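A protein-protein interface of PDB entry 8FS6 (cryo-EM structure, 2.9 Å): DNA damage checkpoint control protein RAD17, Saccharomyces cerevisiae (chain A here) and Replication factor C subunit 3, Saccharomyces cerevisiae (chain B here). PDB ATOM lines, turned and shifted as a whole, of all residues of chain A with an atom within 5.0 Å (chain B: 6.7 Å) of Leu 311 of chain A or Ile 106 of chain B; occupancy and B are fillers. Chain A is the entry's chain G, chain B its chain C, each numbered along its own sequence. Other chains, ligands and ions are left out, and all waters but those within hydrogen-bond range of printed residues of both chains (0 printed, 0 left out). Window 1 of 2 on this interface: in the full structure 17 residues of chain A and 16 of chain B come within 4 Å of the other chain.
Printed residues of chain A that touch a printed residue of chain B: Val 55, Gly 144, Gly 263, Leu 311, Glu 312 and Lys 313.
Hydrophobic or aromatic side chains of chain A that line the printed part of chain B: Val 55 and Leu 311.
Along chain A the printed residues that touch a printed residue of chain B span positions 55 to 313.
Along chain B the printed residues that touch a printed residue of chain A span positions 77 to 106.
Among the printed residues, 8 pairs touch across the chains.
Among the printed residues, Asp or Glu carboxylates within 4 Å of a Lys or Arg side-chain nitrogen of the other chain: Glu 312 of chain A with Arg 104 of chain B.
Of chain A, only Gly 144 (3.2 Å) and Leu 311 (3.8 Å) come within 4 Å of Ile 106 of chain B.
Printed residues of chain A within 4 Å of Asn 77 of chain B: Gly 144 (3.3 Å).
Of the printed residues of chain B, Val 55 of chain A touches Thr 103 (3.5 Å).
Of the printed residues of chain A, Thr 103 of chain B touches Val 55 and Glu 312.
Of the printed residues of chain B, Lys 313 of chain A touches Arg 104 (3.3 Å).
Lys 112 of chain B touches none of the printed residues of chain A.
The nearest residue of chain B that does not touch Leu 311 of chain A is Thr 103 of chain B (4.1 Å).
The nearest printed residue of chain A that does not touch Asn 77 of chain B is His 54 of chain A (4.8 Å).
OG1 of Thr 103 of chain B touches CG1 of Val 55 of chain A (3.5 Å).
Gly 144 of chain A touches Asn 77 of chain B.
O of Gly 144 of chain A touches CG2 of Ile 106 of chain B, at 3.2 Å.
Ile 106 of chain B touches Leu 311 of chain A (CD1 to CD1, 3.8 Å).
Thr 103 of chain B touches Glu 312 of chain A.
Lys 313 of chain A touches Arg 104 of chain B.
NH2 of Arg 104 of chain B lies within salt-bridge range of OE1 of Glu 312 of chain A (3.6 Å).
N of Gly 263 of chain A sits close to NH2 of Arg 104 of chain B, at 3.1 Å.
The side-chain amide oxygen (OD1) of Asn 77 of chain B lies close to the backbone carbonyl oxygen (O) of Asn 74 of chain B (2.9 Å).
N of Ile 106 of chain B lies close to SD of Met 78 of chain B (3.7 Å).
The side-chain hydroxyl (OG1) of Thr 103 of chain B lies within hydrogen-bond range of the backbone carbonyl oxygen (O) of Phe 100 of chain B (3.4 Å).
OG1 of Thr 103 of chain B lies within hydrogen-bond range of NZ of Lys 112 of chain B.
The backbone carbonyl oxygen (O) of Val 55 of chain A is in hydrogen-bond range of the backbone NH (N) of Leu 311 of chain A (3.1 Å).
The backbone carbonyl oxygen (O) of Gly 263 of chain A is in hydrogen-bond range of the backbone NH (N) of Glu 312 of chain A (2.6 Å).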
ATOM      1  N   HIS A  54      28.185  11.789  -7.703  1.00  0.00           N
ATOM      2  CA  HIS A  54      28.262  11.801  -9.164  1.00  0.00           C
ATOM      3  C   HIS A  54      27.501  10.641  -9.805  1.00  0.00           C
ATOM      4  O   HIS A  54      27.783  10.268 -10.948  1.00  0.00           O
ATOM      5  CB  HIS A  54      29.716  11.803  -9.654  1.00  0.00           C
ATOM      6  CG  HIS A  54      30.622  12.691  -8.859  1.00  0.00           C
ATOM      7  ND1 HIS A  54      31.300  12.255  -7.742  1.00  0.00           N
ATOM      8  CD2 HIS A  54      30.965  13.991  -9.023  1.00  0.00           C
ATOM      9  CE1 HIS A  54      32.020  13.248  -7.250  1.00  0.00           C
ATOM     10  NE2 HIS A  54      31.835  14.312  -8.010  1.00  0.00           N
ATOM     11  N   VAL A  55      26.538  10.059  -9.094  1.00  0.00           N
ATOM     12  CA  VAL A  55      25.755   8.952  -9.623  1.00  0.00           C
ATOM     13  C   VAL A  55      24.279   9.297  -9.770  1.00  0.00           C
ATOM     14  O   VAL A  55      23.564   8.584 -10.491  1.00  0.00           O
ATOM     15  CB  VAL A  55      25.920   7.684  -8.760  1.00  0.00           C
ATOM     16  CG1 VAL A  55      27.372   7.235  -8.750  1.00  0.00           C
ATOM     17  CG2 VAL A  55      25.420   7.931  -7.346  1.00  0.00           C
ATOM     18  N   GLY A 144      27.113  16.362 -17.084  1.00  0.00           N
ATOM     19  CA  GLY A 144      27.530  14.970 -17.141  1.00  0.00           C
ATOM     20  C   GLY A 144      26.392  14.006 -16.869  1.00  0.00           C
ATOM     21  O   GLY A 144      26.200  13.029 -17.596  1.00  0.00           O
ATOM     22  N   LEU A 145      25.609  14.278 -15.824  1.00  0.00           N
ATOM     23  CA  LEU A 145      24.482  13.421 -15.454  1.00  0.00           C
ATOM     24  C   LEU A 145      23.242  13.842 -16.243  1.00  0.00           C
ATOM     25  O   LEU A 145      22.238  14.311 -15.702  1.00  0.00           O
ATOM     26  CB  LEU A 145      24.237  13.480 -13.953  1.00  0.00           C
ATOM     27  CG  LEU A 145      24.987  12.460 -13.096  1.00  0.00           C
ATOM     28  CD1 LEU A 145      25.221  13.007 -11.697  1.00  0.00           C
ATOM     29  CD2 LEU A 145      24.215  11.155 -13.038  1.00  0.00           C
ATOM     30  N   PHE A 237      19.689  -0.807 -11.395  1.00  0.00           N
ATOM     31  CA  PHE A 237      19.919   0.403 -10.622  1.00  0.00           C
ATOM     32  C   PHE A 237      19.975   0.071  -9.140  1.00  0.00           C
ATOM     33  O   PHE A 237      19.181  -0.734  -8.643  1.00  0.00           O
ATOM     34  CB  PHE A 237      18.822   1.440 -10.876  1.00  0.00           C
ATOM     35  CG  PHE A 237      18.721   1.876 -12.307  1.00  0.00           C
ATOM     36  CD1 PHE A 237      19.512   2.903 -12.789  1.00  0.00           C
ATOM     37  CD2 PHE A 237      17.835   1.255 -13.171  1.00  0.00           C
ATOM     38  CE1 PHE A 237      19.421   3.305 -14.105  1.00  0.00           C
ATOM     39  CE2 PHE A 237      17.739   1.653 -14.488  1.00  0.00           C
ATOM     40  CZ  PHE A 237      18.535   2.677 -14.955  1.00  0.00           C
ATOM     41  N   GLY A 263      23.252   3.637 -20.069  1.00  0.00           N
ATOM     42  CA  GLY A 263      22.960   3.398 -18.670  1.00  0.00           C
ATOM     43  C   GLY A 263      22.721   4.617 -17.803  1.00  0.00           C
ATOM     44  O   GLY A 263      23.257   4.703 -16.694  1.00  0.00           O
ATOM     45  N   VAL A 264      21.927   5.569 -18.286  1.00  0.00           N
ATOM     46  CA  VAL A 264      21.455   6.683 -17.471  1.00  0.00           C
ATOM     47  C   VAL A 264      19.933   6.724 -17.565  1.00  0.00           C
ATOM     48  O   VAL A 264      19.362   6.515 -18.642  1.00  0.00           O
ATOM     49  CB  VAL A 264      22.096   8.022 -17.882  1.00  0.00           C
ATOM     50  CG1 VAL A 264      21.654   8.461 -19.261  1.00  0.00           C
ATOM     51  CG2 VAL A 264      21.785   9.104 -16.853  1.00  0.00           C
ATOM     52  N   LEU A 265      19.280   6.937 -16.425  1.00  0.00           N
ATOM     53  CA  LEU A 265      17.826   6.981 -16.340  1.00  0.00           C
ATOM     54  C   LEU A 265      17.387   8.371 -15.907  1.00  0.00           C
ATOM     55  O   LEU A 265      17.926   8.924 -14.945  1.00  0.00           O
ATOM     56  CB  LEU A 265      17.308   5.935 -15.352  1.00  0.00           C
ATOM     57  CG  LEU A 265      15.794   5.833 -15.151  1.00  0.00           C
ATOM     58  CD1 LEU A 265      15.090   5.515 -16.460  1.00  0.00           C
ATOM     59  CD2 LEU A 265      15.467   4.791 -14.095  1.00  0.00           C
ATOM     60  N   CYS A 309      18.065  12.502 -12.731  1.00  0.00           N
ATOM     61  CA  CYS A 309      18.903  11.642 -13.552  1.00  0.00           C
ATOM     62  C   CYS A 309      19.650  10.639 -12.679  1.00  0.00           C
ATOM     63  O   CYS A 309      20.137  10.970 -11.596  1.00  0.00           O
ATOM     64  CB  CYS A 309      19.892  12.473 -14.367  1.00  0.00           C
ATOM     65  SG  CYS A 309      19.241  13.058 -15.949  1.00  0.00           S
ATOM     66  N   MET A 310      19.738   9.403 -13.166  1.00  0.00           N
ATOM     67  CA  MET A 310      20.302   8.310 -12.387  1.00  0.00           C
ATOM     68  C   MET A 310      21.155   7.426 -13.283  1.00  0.00           C
ATOM     69  O   MET A 310      20.789   7.163 -14.429  1.00  0.00           O
ATOM     70  CB  MET A 310      19.195   7.475 -11.735  1.00  0.00           C
ATOM     71  CG  MET A 310      19.653   6.633 -10.562  1.00  0.00           C
ATOM     72  SD  MET A 310      18.276   5.850  -9.701  1.00  0.00           S
ATOM     73  CE  MET A 310      16.906   6.902 -10.179  1.00  0.00           C
ATOM     74  N   LEU A 311      22.278   6.954 -12.746  1.00  0.00           N
ATOM     75  CA  LEU A 311      23.201   6.097 -13.478  1.00  0.00           C
ATOM     76  C   LEU A 311      22.915   4.628 -13.192  1.00  0.00           C
ATOM     77  O   LEU A 311      22.554   4.260 -12.070  1.00  0.00           O
ATOM     78  CB  LEU A 311      24.654   6.417 -13.116  1.00  0.00           C
ATOM     79  CG  LEU A 311      25.254   7.694 -13.706  1.00  0.00           C
ATOM     80  CD1 LEU A 311      26.663   7.914 -13.180  1.00  0.00           C
ATOM     81  CD2 LEU A 311      25.248   7.641 -15.225  1.00  0.00           C
ATOM     82  N   GLU A 312      23.079   3.796 -14.217  1.00  0.00           N
ATOM     83  CA  GLU A 312      22.886   2.360 -14.089  1.00  0.00           C
ATOM     84  C   GLU A 312      24.149   1.698 -13.548  1.00  0.00           C
ATOM     85  O   GLU A 312      25.267   2.170 -13.771  1.00  0.00           O
ATOM     86  CB  GLU A 312      22.505   1.758 -15.446  1.00  0.00           C
ATOM     87  CG  GLU A 312      22.160   0.276 -15.430  1.00  0.00           C
ATOM     88  CD  GLU A 312      21.820  -0.268 -16.804  1.00  0.00           C
ATOM     89  OE1 GLU A 312      21.859   0.508 -17.780  1.00  0.00           O
ATOM     90  OE2 GLU A 312      21.516  -1.475 -16.907  1.00  0.00           O
ATOM     91  N   LYS A 313      23.960   0.605 -12.811  1.00  0.00           N
ATOM     92  CA  LYS A 313      25.088  -0.184 -12.341  1.00  0.00           C
ATOM     93  C   LYS A 313      25.714  -0.959 -13.500  1.00  0.00           C
ATOM     94  O   LYS A 313      25.088  -1.195 -14.536  1.00  0.00           O
ATOM     95  CB  LYS A 313      24.648  -1.147 -11.237  1.00  0.00           C
ATOM     96  CG  LYS A 313      23.875  -0.482 -10.109  1.00  0.00           C
ATOM     97  CD  LYS A 313      24.778  -0.163  -8.930  1.00  0.00           C
ATOM     98  CE  LYS A 313      25.279  -1.432  -8.263  1.00  0.00           C
ATOM     99  NZ  LYS A 313      24.157  -2.326  -7.865  1.00  0.00           N
ATOM    100  N   ASN B  74      35.795  15.890 -19.636  1.00  0.00           N
ATOM    101  CA  ASN B  74      35.027  15.037 -18.736  1.00  0.00           C
ATOM    102  C   ASN B  74      35.791  14.719 -17.454  1.00  0.00           C
ATOM    103  O   ASN B  74      35.612  13.642 -16.874  1.00  0.00           O
ATOM    104  CB  ASN B  74      34.606  13.748 -19.442  1.00  0.00           C
ATOM    105  CG  ASN B  74      34.454  13.923 -20.941  1.00  0.00           C
ATOM    106  OD1 ASN B  74      33.451  14.453 -21.418  1.00  0.00           O
ATOM    107  ND2 ASN B  74      35.453  13.476 -21.692  1.00  0.00           N
ATOM    108  N   ASN B  77      33.210  14.649 -14.041  1.00  0.00           N
ATOM    109  CA  ASN B  77      32.279  13.552 -13.818  1.00  0.00           C
ATOM    110  C   ASN B  77      32.935  12.179 -13.878  1.00  0.00           C
ATOM    111  O   ASN B  77      32.239  11.171 -13.719  1.00  0.00           O
ATOM    112  CB  ASN B  77      31.135  13.618 -14.836  1.00  0.00           C
ATOM    113  CG  ASN B  77      31.624  13.896 -16.242  1.00  0.00           C
ATOM    114  OD1 ASN B  77      32.817  14.081 -16.470  1.00  0.00           O
ATOM    115  ND2 ASN B  77      30.700  13.924 -17.194  1.00  0.00           N
ATOM    116  N   MET B  78      34.247  12.107 -14.100  1.00  0.00           N
ATOM    117  CA  MET B  78      34.941  10.828 -14.195  1.00  0.00           C
ATOM    118  C   MET B  78      36.113  10.713 -13.230  1.00  0.00           C
ATOM    119  O   MET B  78      36.835   9.710 -13.268  1.00  0.00           O
ATOM    120  CB  MET B  78      35.423  10.585 -15.628  1.00  0.00           C
ATOM    121  CG  MET B  78      34.300  10.392 -16.628  1.00  0.00           C
ATOM    122  SD  MET B  78      33.486   8.800 -16.403  1.00  0.00           S
ATOM    123  CE  MET B  78      33.917   7.984 -17.934  1.00  0.00           C
ATOM    124  N   PHE B 100      30.703   4.742  -6.774  1.00  0.00           N
ATOM    125  CA  PHE B 100      31.331   5.411  -7.907  1.00  0.00           C
ATOM    126  C   PHE B 100      31.990   4.403  -8.836  1.00  0.00           C
ATOM    127  O   PHE B 100      31.987   4.589 -10.058  1.00  0.00           O
ATOM    128  CB  PHE B 100      32.353   6.441  -7.425  1.00  0.00           C
ATOM    129  CG  PHE B 100      32.954   7.262  -8.532  1.00  0.00           C
ATOM    130  CD1 PHE B 100      32.276   8.355  -9.048  1.00  0.00           C
ATOM    131  CD2 PHE B 100      34.196   6.942  -9.056  1.00  0.00           C
ATOM    132  CE1 PHE B 100      32.827   9.111 -10.068  1.00  0.00           C
ATOM    133  CE2 PHE B 100      34.750   7.694 -10.074  1.00  0.00           C
ATOM    134  CZ  PHE B 100      34.065   8.780 -10.580  1.00  0.00           C
ATOM    135  N   THR B 103      28.837   2.087 -10.688  1.00  0.00           N
ATOM    136  CA  THR B 103      28.027   2.676 -11.746  1.00  0.00           C
ATOM    137  C   THR B 103      28.794   2.724 -13.063  1.00  0.00           C
ATOM    138  O   THR B 103      30.025   2.802 -13.091  1.00  0.00           O
ATOM    139  CB  THR B 103      27.573   4.082 -11.353  1.00  0.00           C
ATOM    140  OG1 THR B 103      28.686   4.819 -10.833  1.00  0.00           O
ATOM    141  CG2 THR B 103      26.478   4.008 -10.299  1.00  0.00           C
ATOM    142  N   ARG B 104      28.046   2.673 -14.163  1.00  0.00           N
ATOM    143  CA  ARG B 104      28.646   2.642 -15.487  1.00  0.00           C
ATOM    144  C   ARG B 104      29.302   3.979 -15.823  1.00  0.00           C
ATOM    145  O   ARG B 104      28.995   5.023 -15.242  1.00  0.00           O
ATOM    146  CB  ARG B 104      27.599   2.295 -16.548  1.00  0.00           C
ATOM    147  CG  ARG B 104      26.846   1.004 -16.278  1.00  0.00           C
ATOM    148  CD  ARG B 104      26.702   0.158 -17.533  1.00  0.00           C
ATOM    149  NE  ARG B 104      25.832   0.780 -18.523  1.00  0.00           N
ATOM    150  CZ  ARG B 104      25.132   0.110 -19.428  1.00  0.00           C
ATOM    151  NH1 ARG B 104      25.170  -1.211 -19.492  1.00  0.00           N
ATOM    152  NH2 ARG B 104      24.373   0.783 -20.290  1.00  0.00           N
ATOM    153  N   GLN B 105      30.224   3.926 -16.780  1.00  0.00           N
ATOM    154  CA  GLN B 105      30.956   5.109 -17.208  1.00  0.00           C
ATOM    155  C   GLN B 105      30.024   6.099 -17.897  1.00  0.00           C
ATOM    156  O   GLN B 105      29.059   5.721 -18.564  1.00  0.00           O
ATOM    157  CB  GLN B 105      32.096   4.717 -18.151  1.00  0.00           C
ATOM    158  CG  GLN B 105      31.769   3.570 -19.102  1.00  0.00           C
ATOM    159  CD  GLN B 105      32.056   2.204 -18.504  1.00  0.00           C
ATOM    160  OE1 GLN B 105      33.069   2.005 -17.834  1.00  0.00           O
ATOM    161  NE2 GLN B 105      31.159   1.254 -18.745  1.00  0.00           N
ATOM    162  N   ILE B 106      30.324   7.384 -17.727  1.00  0.00           N
ATOM    163  CA  ILE B 106      29.466   8.452 -18.269  1.00  0.00           C
ATOM    164  C   ILE B 106      30.083   8.868 -19.599  1.00  0.00           C
ATOM    165  O   ILE B 106      30.937   9.753 -19.688  1.00  0.00           O
ATOM    166  CB  ILE B 106      29.311   9.623 -17.294  1.00  0.00           C
ATOM    167  CG1 ILE B 106      29.379   9.129 -15.848  1.00  0.00           C
ATOM    168  CG2 ILE B 106      28.001  10.346 -17.548  1.00  0.00           C
ATOM    169  CD1 ILE B 106      29.152  10.220 -14.820  1.00  0.00           C
ATOM    170  N   PHE B 107      29.648   8.193 -20.662  1.00  0.00           N
ATOM    171  CA  PHE B 107      29.859   8.559 -22.062  1.00  0.00           C
ATOM    172  C   PHE B 107      31.297   8.479 -22.549  1.00  0.00           C
ATOM    173  O   PHE B 107      31.534   8.719 -23.738  1.00  0.00           O
ATOM    174  CB  PHE B 107      29.366   9.975 -22.378  1.00  0.00           C
ATOM    175  CG  PHE B 107      27.995  10.014 -22.941  1.00  0.00           C
ATOM    176  CD1 PHE B 107      27.723   9.373 -24.136  1.00  0.00           C
ATOM    177  CD2 PHE B 107      26.982  10.703 -22.302  1.00  0.00           C
ATOM    178  CE1 PHE B 107      26.470   9.399 -24.674  1.00  0.00           C
ATOM    179  CE2 PHE B 107      25.721  10.734 -22.841  1.00  0.00           C
ATOM    180  CZ  PHE B 107      25.475  10.085 -24.033  1.00  0.00           C
ATOM    181  N   SER B 108      32.262   8.157 -21.694  1.00  0.00           N
ATOM    182  CA  SER B 108      33.647   8.194 -22.139  1.00  0.00           C
ATOM    183  C   SER B 108      34.101   6.899 -22.795  1.00  0.00           C
ATOM    184  O   SER B 108      35.195   6.874 -23.369  1.00  0.00           O
ATOM    185  CB  SER B 108      34.567   8.521 -20.962  1.00  0.00           C
ATOM    186  OG  SER B 108      35.906   8.676 -21.395  1.00  0.00           O
ATOM    187  N   LYS B 109      33.309   5.828 -22.704  1.00  0.00           N
ATOM    188  CA  LYS B 109      33.578   4.504 -23.262  1.00  0.00           C
ATOM    189  C   LYS B 109      34.785   3.832 -22.610  1.00  0.00           C
ATOM    190  O   LYS B 109      35.108   2.689 -22.956  1.00  0.00           O
ATOM    191  CB  LYS B 109      33.769   4.543 -24.790  1.00  0.00           C
ATOM    192  CG  LYS B 109      33.496   3.230 -25.515  1.00  0.00           C
ATOM    193  CD  LYS B 109      32.072   2.753 -25.290  1.00  0.00           C
ATOM    194  CE  LYS B 109      31.092   3.499 -26.178  1.00  0.00           C
ATOM    195  NZ  LYS B 109      31.275   3.155 -27.615  1.00  0.00           N
ATOM    196  N   GLY B 110      35.451   4.489 -21.664  1.00  0.00           N
ATOM    197  CA  GLY B 110      36.604   3.913 -21.005  1.00  0.00           C
ATOM    198  C   GLY B 110      36.369   3.645 -19.534  1.00  0.00           C
ATOM    199  O   GLY B 110      35.279   3.222 -19.138  1.00  0.00           O
ATOM    200  N   LYS B 112      36.754   4.791 -15.257  1.00  0.00           N
ATOM    201  CA  LYS B 112      36.720   5.893 -14.309  1.00  0.00           C
ATOM    202  C   LYS B 112      37.992   5.886 -13.469  1.00  0.00           C
ATOM    203  O   LYS B 112      38.697   4.878 -13.376  1.00  0.00           O
ATOM    204  CB  LYS B 112      35.488   5.799 -13.407  1.00  0.00           C
ATOM    205  CG  LYS B 112      34.283   5.155 -14.074  1.00  0.00           C
ATOM    206  CD  LYS B 112      33.111   5.038 -13.114  1.00  0.00           C
ATOM    207  CE  LYS B 112      32.414   6.375 -12.925  1.00  0.00           C
ATOM    208  NZ  LYS B 112      31.128   6.229 -12.190  1.00  0.00           N
